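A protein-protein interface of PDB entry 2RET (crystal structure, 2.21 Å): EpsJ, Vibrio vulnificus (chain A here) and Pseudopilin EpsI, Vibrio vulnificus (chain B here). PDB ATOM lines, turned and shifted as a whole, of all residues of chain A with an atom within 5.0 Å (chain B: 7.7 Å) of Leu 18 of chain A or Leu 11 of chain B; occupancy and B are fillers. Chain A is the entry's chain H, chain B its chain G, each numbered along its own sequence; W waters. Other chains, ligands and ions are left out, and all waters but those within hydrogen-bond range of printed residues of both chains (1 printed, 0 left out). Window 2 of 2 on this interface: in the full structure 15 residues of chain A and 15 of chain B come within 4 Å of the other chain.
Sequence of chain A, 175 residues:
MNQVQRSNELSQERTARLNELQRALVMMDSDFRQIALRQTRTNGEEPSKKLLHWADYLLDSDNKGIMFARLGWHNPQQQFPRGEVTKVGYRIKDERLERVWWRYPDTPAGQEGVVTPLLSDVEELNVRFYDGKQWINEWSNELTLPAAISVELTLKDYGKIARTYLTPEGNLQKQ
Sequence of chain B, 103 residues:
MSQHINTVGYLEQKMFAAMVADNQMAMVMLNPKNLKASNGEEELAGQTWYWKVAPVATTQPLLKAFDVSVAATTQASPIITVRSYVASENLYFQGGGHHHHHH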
ATOM      1  N   ARG A  14     -15.490 -21.254  -0.433  1.00  0.00           N
ATOM      2  CA  ARG A  14     -16.750 -20.547  -0.685  1.00  0.00           C
ATOM      3  C   ARG A  14     -17.718 -20.637   0.496  1.00  0.00           C
ATOM      4  O   ARG A  14     -18.385 -19.633   0.857  1.00  0.00           O
ATOM      5  CB  ARG A  14     -17.437 -21.071  -1.923  1.00  0.00           C
ATOM      6  CG  ARG A  14     -16.608 -20.926  -3.179  1.00  0.00           C
ATOM      7  CD  ARG A  14     -17.377 -20.170  -4.246  1.00  0.00           C
ATOM      8  NE  ARG A  14     -17.274 -20.747  -5.596  1.00  0.00           N
ATOM      9  CZ  ARG A  14     -17.886 -21.857  -6.011  1.00  0.00           C
ATOM     10  NH1 ARG A  14     -18.641 -22.589  -5.186  1.00  0.00           N
ATOM     11  NH2 ARG A  14     -17.722 -22.253  -7.264  1.00  0.00           N
ATOM     12  N   THR A  15     -17.804 -21.840   1.062  1.00  0.00           N
ATOM     13  CA  THR A  15     -18.621 -22.102   2.234  1.00  0.00           C
ATOM     14  C   THR A  15     -18.081 -21.350   3.438  1.00  0.00           C
ATOM     15  O   THR A  15     -18.855 -20.794   4.200  1.00  0.00           O
ATOM     16  CB  THR A  15     -18.662 -23.601   2.587  1.00  0.00           C
ATOM     17  OG1 THR A  15     -18.970 -24.367   1.413  1.00  0.00           O
ATOM     18  CG2 THR A  15     -19.690 -23.869   3.676  1.00  0.00           C
ATOM     19  N   ALA A  16     -16.760 -21.337   3.612  1.00  0.00           N
ATOM     20  CA  ALA A  16     -16.148 -20.594   4.727  1.00  0.00           C
ATOM     21  C   ALA A  16     -16.485 -19.113   4.621  1.00  0.00           C
ATOM     22  O   ALA A  16     -16.776 -18.479   5.624  1.00  0.00           O
ATOM     23  CB  ALA A  16     -14.626 -20.796   4.777  1.00  0.00           C
ATOM     24  N   ARG A  17     -16.440 -18.583   3.407  1.00  0.00           N
ATOM     25  CA  ARG A  17     -16.738 -17.185   3.127  1.00  0.00           C
ATOM     26  C   ARG A  17     -18.209 -16.876   3.426  1.00  0.00           C
ATOM     27  O   ARG A  17     -18.537 -15.887   4.074  1.00  0.00           O
ATOM     28  CB  ARG A  17     -16.421 -16.866   1.652  1.00  0.00           C
ATOM     29  CG  ARG A  17     -16.865 -15.477   1.176  1.00  0.00           C
ATOM     30  CD  ARG A  17     -16.315 -14.372   2.108  1.00  0.00           C
ATOM     31  NE  ARG A  17     -16.276 -13.062   1.461  1.00  0.00           N
ATOM     32  CZ  ARG A  17     -15.732 -11.984   1.998  1.00  0.00           C
ATOM     33  NH1 ARG A  17     -15.224 -12.044   3.190  1.00  0.00           N
ATOM     34  NH2 ARG A  17     -15.715 -10.839   1.333  1.00  0.00           N
ATOM     35  N   LEU A  18     -19.095 -17.746   2.962  1.00  0.00           N
ATOM     36  CA  LEU A  18     -20.512 -17.615   3.265  1.00  0.00           C
ATOM     37  C   LEU A  18     -20.749 -17.588   4.791  1.00  0.00           C
ATOM     38  O   LEU A  18     -21.434 -16.692   5.304  1.00  0.00           O
ATOM     39  CB  LEU A  18     -21.258 -18.760   2.583  1.00  0.00           C
ATOM     40  CG  LEU A  18     -22.743 -18.705   2.228  1.00  0.00           C
ATOM     41  CD1 LEU A  18     -23.561 -19.452   3.283  1.00  0.00           C
ATOM     42  CD2 LEU A  18     -23.220 -17.271   2.009  1.00  0.00           C
ATOM     43  N   ASN A  19     -20.152 -18.546   5.508  1.00  0.00           N
ATOM     44  CA  ASN A  19     -20.280 -18.628   6.967  1.00  0.00           C
ATOM     45  C   ASN A  19     -19.733 -17.400   7.683  1.00  0.00           C
ATOM     46  O   ASN A  19     -20.333 -16.904   8.621  1.00  0.00           O
ATOM     47  CB  ASN A  19     -19.598 -19.890   7.505  1.00  0.00           C
ATOM     48  CG  ASN A  19     -20.307 -21.170   7.086  1.00  0.00           C
ATOM     49  OD1 ASN A  19     -21.421 -21.142   6.565  1.00  0.00           O
ATOM     50  ND2 ASN A  19     -19.657 -22.297   7.309  1.00  0.00           N
ATOM     51  N   GLU A  20     -18.588 -16.916   7.216  1.00  0.00           N
ATOM     52  CA  GLU A  20     -17.993 -15.686   7.694  1.00  0.00           C
ATOM     53  C   GLU A  20     -18.948 -14.516   7.530  1.00  0.00           C
ATOM     54  O   GLU A  20     -19.113 -13.711   8.439  1.00  0.00           O
ATOM     55  CB  GLU A  20     -16.710 -15.404   6.906  1.00  0.00           C
ATOM     56  CG  GLU A  20     -16.027 -14.083   7.280  1.00  0.00           C
ATOM     57  CD  GLU A  20     -14.876 -13.716   6.358  1.00  0.00           C
ATOM     58  OE1 GLU A  20     -14.811 -14.241   5.230  1.00  0.00           O
ATOM     59  OE2 GLU A  20     -14.030 -12.902   6.768  1.00  0.00           O
ATOM     60  N   LEU A  21     -19.537 -14.415   6.335  1.00  0.00           N
ATOM     61  CA  LEU A  21     -20.504 -13.374   6.030  1.00  0.00           C
ATOM     62  C   LEU A  21     -21.691 -13.423   6.992  1.00  0.00           C
ATOM     63  O   LEU A  21     -22.063 -12.414   7.587  1.00  0.00           O
ATOM     64  CB  LEU A  21     -20.953 -13.467   4.571  1.00  0.00           C
ATOM     65  CG  LEU A  21     -21.874 -12.371   3.996  1.00  0.00           C
ATOM     66  CD1 LEU A  21     -21.555 -10.966   4.583  1.00  0.00           C
ATOM     67  CD2 LEU A  21     -21.767 -12.403   2.465  1.00  0.00           C
ATOM     68  N   GLN A  22     -22.253 -14.610   7.154  1.00  0.00           N
ATOM     69  CA  GLN A  22     -23.304 -14.872   8.143  1.00  0.00           C
ATOM     70  C   GLN A  22     -22.999 -14.472   9.581  1.00  0.00           C
ATOM     71  O   GLN A  22     -23.865 -13.960  10.279  1.00  0.00           O
ATOM     72  CB  GLN A  22     -23.641 -16.366   8.129  1.00  0.00           C
ATOM     73  CG  GLN A  22     -25.020 -16.613   7.642  1.00  0.00           C
ATOM     74  CD  GLN A  22     -25.269 -18.024   7.216  1.00  0.00           C
ATOM     75  OE1 GLN A  22     -26.151 -18.260   6.394  1.00  0.00           O
ATOM     76  NE2 GLN A  22     -24.517 -18.969   7.750  1.00  0.00           N
ATOM     77  N   TYR A 158     -18.624 -10.337  -3.575  1.00  0.00           N
ATOM     78  CA  TYR A 158     -20.071 -10.346  -3.709  1.00  0.00           C
ATOM     79  C   TYR A 158     -20.625  -9.021  -4.195  1.00  0.00           C
ATOM     80  O   TYR A 158     -21.783  -8.956  -4.678  1.00  0.00           O
ATOM     81  CB  TYR A 158     -20.717 -10.755  -2.391  1.00  0.00           C
ATOM     82  CG  TYR A 158     -20.646 -12.250  -2.154  1.00  0.00           C
ATOM     83  CD1 TYR A 158     -21.405 -13.109  -2.906  1.00  0.00           C
ATOM     84  CD2 TYR A 158     -19.815 -12.797  -1.185  1.00  0.00           C
ATOM     85  CE1 TYR A 158     -21.352 -14.465  -2.720  1.00  0.00           C
ATOM     86  CE2 TYR A 158     -19.771 -14.170  -0.969  1.00  0.00           C
ATOM     87  CZ  TYR A 158     -20.534 -14.996  -1.744  1.00  0.00           C
ATOM     88  OH  TYR A 158     -20.497 -16.379  -1.573  1.00  0.00           O
ATOM     89  N   THR B   7     -24.752 -26.546  -3.272  1.00  0.00           N
ATOM     90  CA  THR B   7     -25.139 -26.305  -1.857  1.00  0.00           C
ATOM     91  C   THR B   7     -24.885 -24.832  -1.461  1.00  0.00           C
ATOM     92  O   THR B   7     -25.787 -24.158  -0.940  1.00  0.00           O
ATOM     93  CB  THR B   7     -24.488 -27.363  -0.850  1.00  0.00           C
ATOM     94  OG1 THR B   7     -24.721 -26.966   0.506  1.00  0.00           O
ATOM     95  CG2 THR B   7     -22.968 -27.566  -1.058  1.00  0.00           C
ATOM     96  N   VAL B   8     -23.695 -24.308  -1.745  1.00  0.00           N
ATOM     97  CA  VAL B   8     -23.413 -22.910  -1.407  1.00  0.00           C
ATOM     98  C   VAL B   8     -24.241 -21.928  -2.276  1.00  0.00           C
ATOM     99  O   VAL B   8     -24.634 -20.872  -1.801  1.00  0.00           O
ATOM    100  CB  VAL B   8     -21.914 -22.591  -1.469  1.00  0.00           C
ATOM    101  CG1 VAL B   8     -21.406 -22.740  -2.879  1.00  0.00           C
ATOM    102  CG2 VAL B   8     -21.637 -21.190  -0.971  1.00  0.00           C
ATOM    103  N   GLY B   9     -24.513 -22.288  -3.528  1.00  0.00           N
ATOM    104  CA  GLY B   9     -25.311 -21.457  -4.433  1.00  0.00           C
ATOM    105  C   GLY B   9     -26.699 -21.179  -3.876  1.00  0.00           C
ATOM    106  O   GLY B   9     -27.203 -20.060  -3.940  1.00  0.00           O
ATOM    107  N   TYR B  10     -27.317 -22.231  -3.350  1.00  0.00           N
ATOM    108  CA  TYR B  10     -28.637 -22.128  -2.737  1.00  0.00           C
ATOM    109  C   TYR B  10     -28.573 -21.337  -1.440  1.00  0.00           C
ATOM    110  O   TYR B  10     -29.404 -20.507  -1.182  1.00  0.00           O
ATOM    111  CB  TYR B  10     -29.184 -23.530  -2.477  1.00  0.00           C
ATOM    112  CG  TYR B  10     -30.096 -23.678  -1.275  1.00  0.00           C
ATOM    113  CD1 TYR B  10     -31.424 -23.313  -1.343  1.00  0.00           C
ATOM    114  CD2 TYR B  10     -29.624 -24.234  -0.074  1.00  0.00           C
ATOM    115  CE1 TYR B  10     -32.273 -23.484  -0.249  1.00  0.00           C
ATOM    116  CE2 TYR B  10     -30.473 -24.408   1.039  1.00  0.00           C
ATOM    117  CZ  TYR B  10     -31.797 -24.031   0.938  1.00  0.00           C
ATOM    118  OH  TYR B  10     -32.659 -24.174   2.016  1.00  0.00           O
ATOM    119  N   LEU B  11     -27.571 -21.642  -0.629  1.00  0.00           N
ATOM    120  CA  LEU B  11     -27.323 -20.960   0.635  1.00  0.00           C
ATOM    121  C   LEU B  11     -27.119 -19.462   0.448  1.00  0.00           C
ATOM    122  O   LEU B  11     -27.610 -18.694   1.263  1.00  0.00           O
ATOM    123  CB  LEU B  11     -26.112 -21.585   1.355  1.00  0.00           C
ATOM    124  CG  LEU B  11     -26.229 -23.023   1.894  1.00  0.00           C
ATOM    125  CD1 LEU B  11     -25.040 -23.345   2.807  1.00  0.00           C
ATOM    126  CD2 LEU B  11     -27.560 -23.228   2.653  1.00  0.00           C
ATOM    127  N   GLU B  12     -26.419 -19.052  -0.617  1.00  0.00           N
ATOM    128  CA  GLU B  12     -26.292 -17.627  -0.947  1.00  0.00           C
ATOM    129  C   GLU B  12     -27.627 -16.952  -1.257  1.00  0.00           C
ATOM    130  O   GLU B  12     -27.925 -15.870  -0.754  1.00  0.00           O
ATOM    131  CB  GLU B  12     -25.370 -17.402  -2.130  1.00  0.00           C
ATOM    132  CG  GLU B  12     -23.922 -17.591  -1.822  1.00  0.00           C
ATOM    133  CD  GLU B  12     -23.082 -17.843  -3.066  1.00  0.00           C
ATOM    134  OE1 GLU B  12     -23.639 -17.808  -4.176  1.00  0.00           O
ATOM    135  OE2 GLU B  12     -21.867 -18.079  -2.927  1.00  0.00           O
ATOM    136  N   GLN B  13     -28.406 -17.591  -2.122  1.00  0.00           N
ATOM    137  CA  GLN B  13     -29.714 -17.087  -2.470  1.00  0.00           C
ATOM    138  C   GLN B  13     -30.600 -16.912  -1.227  1.00  0.00           C
ATOM    139  O   GLN B  13     -31.257 -15.917  -1.074  1.00  0.00           O
ATOM    140  CB  GLN B  13     -30.390 -18.007  -3.482  1.00  0.00           C
ATOM    141  CG  GLN B  13     -29.629 -18.123  -4.797  1.00  0.00           C
ATOM    142  CD  GLN B  13     -29.875 -16.971  -5.770  1.00  0.00           C
ATOM    143  OE1 GLN B  13     -28.992 -16.125  -6.014  1.00  0.00           O
ATOM    144  NE2 GLN B  13     -31.066 -16.961  -6.360  1.00  0.00           N
ATOM    145  N   LYS B  14     -30.604 -17.898  -0.350  1.00  0.00           N
ATOM    146  CA  LYS B  14     -31.411 -17.857   0.854  1.00  0.00           C
ATOM    147  C   LYS B  14     -31.027 -16.626   1.723  1.00  0.00           C
ATOM    148  O   LYS B  14     -31.878 -15.822   2.168  1.00  0.00           O
ATOM    149  CB  LYS B  14     -31.192 -19.158   1.604  1.00  0.00           C
ATOM    150  CG  LYS B  14     -32.386 -19.709   2.306  1.00  0.00           C
ATOM    151  CD  LYS B  14     -32.114 -21.116   2.793  1.00  0.00           C
ATOM    152  CE  LYS B  14     -31.310 -21.129   4.093  1.00  0.00           C
ATOM    153  NZ  LYS B  14     -32.173 -21.247   5.325  1.00  0.00           N
ATOM    154  N   MET B  15     -29.719 -16.465   1.902  1.00  0.00           N
ATOM    155  CA  MET B  15     -29.175 -15.416   2.705  1.00  0.00           C
ATOM    156  C   MET B  15     -29.386 -14.023   2.140  1.00  0.00           C
ATOM    157  O   MET B  15     -29.767 -13.105   2.887  1.00  0.00           O
ATOM    158  CB  MET B  15     -27.689 -15.653   2.888  1.00  0.00           C
ATOM    159  CG  MET B  15     -27.003 -14.575   3.756  1.00  0.00           C
ATOM    160  SD  MET B  15     -25.123 -14.991   3.962  1.00  0.00           S
ATOM    161  CE  MET B  15     -25.262 -16.952   3.923  1.00  0.00           C
ATOM    162  N   PHE B  16     -29.128 -13.854   0.840  1.00  0.00           N
ATOM    163  CA  PHE B  16     -29.331 -12.557   0.215  1.00  0.00           C
ATOM    164  C   PHE B  16     -30.837 -12.168   0.015  1.00  0.00           C
ATOM    165  O   PHE B  16     -31.179 -10.994   0.166  1.00  0.00           O
ATOM    166  CB  PHE B  16     -28.569 -12.457  -1.093  1.00  0.00           C
ATOM    167  CG  PHE B  16     -27.074 -12.666  -0.960  1.00  0.00           C
ATOM    168  CD1 PHE B  16     -26.359 -12.109   0.083  1.00  0.00           C
ATOM    169  CD2 PHE B  16     -26.383 -13.409  -1.916  1.00  0.00           C
ATOM    170  CE1 PHE B  16     -24.979 -12.299   0.186  1.00  0.00           C
ATOM    171  CE2 PHE B  16     -25.009 -13.604  -1.817  1.00  0.00           C
ATOM    172  CZ  PHE B  16     -24.306 -13.040  -0.767  1.00  0.00           C
ATOM    173  N   ALA B  17     -31.706 -13.124  -0.328  1.00  0.00           N
ATOM    174  CA  ALA B  17     -33.150 -12.867  -0.366  1.00  0.00           C
ATOM    175  C   ALA B  17     -33.666 -12.446   1.029  1.00  0.00           C
ATOM    176  O   ALA B  17     -34.447 -11.489   1.130  1.00  0.00           O
ATOM    177  CB  ALA B  17     -33.956 -14.113  -0.925  1.00  0.00           C
HETATM  178  O   HOH W   1     -28.127 -19.439   3.766  1.00  0.00           O
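The side-chain carboxylate (OE2) of Glu 12 of chain B lies within hydrogen-bond range of the side-chain hydroxyl (OH) of Tyr 158 of chain A (2.6 Å).
Arg 14 of chain A touches Val 8 of chain B (NH1 to CG1, 3.6 Å).
Leu 18 of chain A touches Leu 11 of chain B.
Leu 18 of chain A touches Glu 12 of chain B.
Leu 18 of chain A touches Met 15 of chain B (CD2 to CE, 2.8 Å).
Phe 16 of chain B touches Leu 21 of chain A.
Gln 22 of chain A touches Met 15 of chain B (OE1 to CE, 2.9 Å).
Tyr 158 of chain A touches Phe 16 of chain B.
Thr 15 of chain A touches none of the printed residues of chain B.
Leu 18 of chain A touches three residues of chain B.
Of the printed residues of chain B, Gln 22 of chain A touches Met 15.
Printed residues of chain A within 4 Å of Val 8 of chain B: Arg 14.
Leu 11 of chain B touches one residue of chain A.
Printed residues of chain A within 4 Å of Met 15 of chain B: Leu 18 and Gln 22.
Of the printed residues of chain A, Phe 16 of chain B touches Leu 21 and Tyr 158.
The nearest residue of chain B that does not touch Leu 18 of chain A is Val 8 of chain B (4.2 Å).
Printed residues of chain A that touch a printed residue of chain B: Arg 14, Leu 18, Leu 21, Gln 22 and Tyr 158.
Hydrophobic or aromatic side chains of chain A within 4 Å of the printed part of chain B: Leu 18, Leu 21 and Tyr 158.
Hydrophobic or aromatic side chains of chain B that line the printed part of chain A: Val 8, Leu 11, Met 15 and Phe 16.
Water W1 bridges O of Leu 11 of chain B (2.7 Å) and OE1 of Gln 22 of chain A (3.5 Å).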
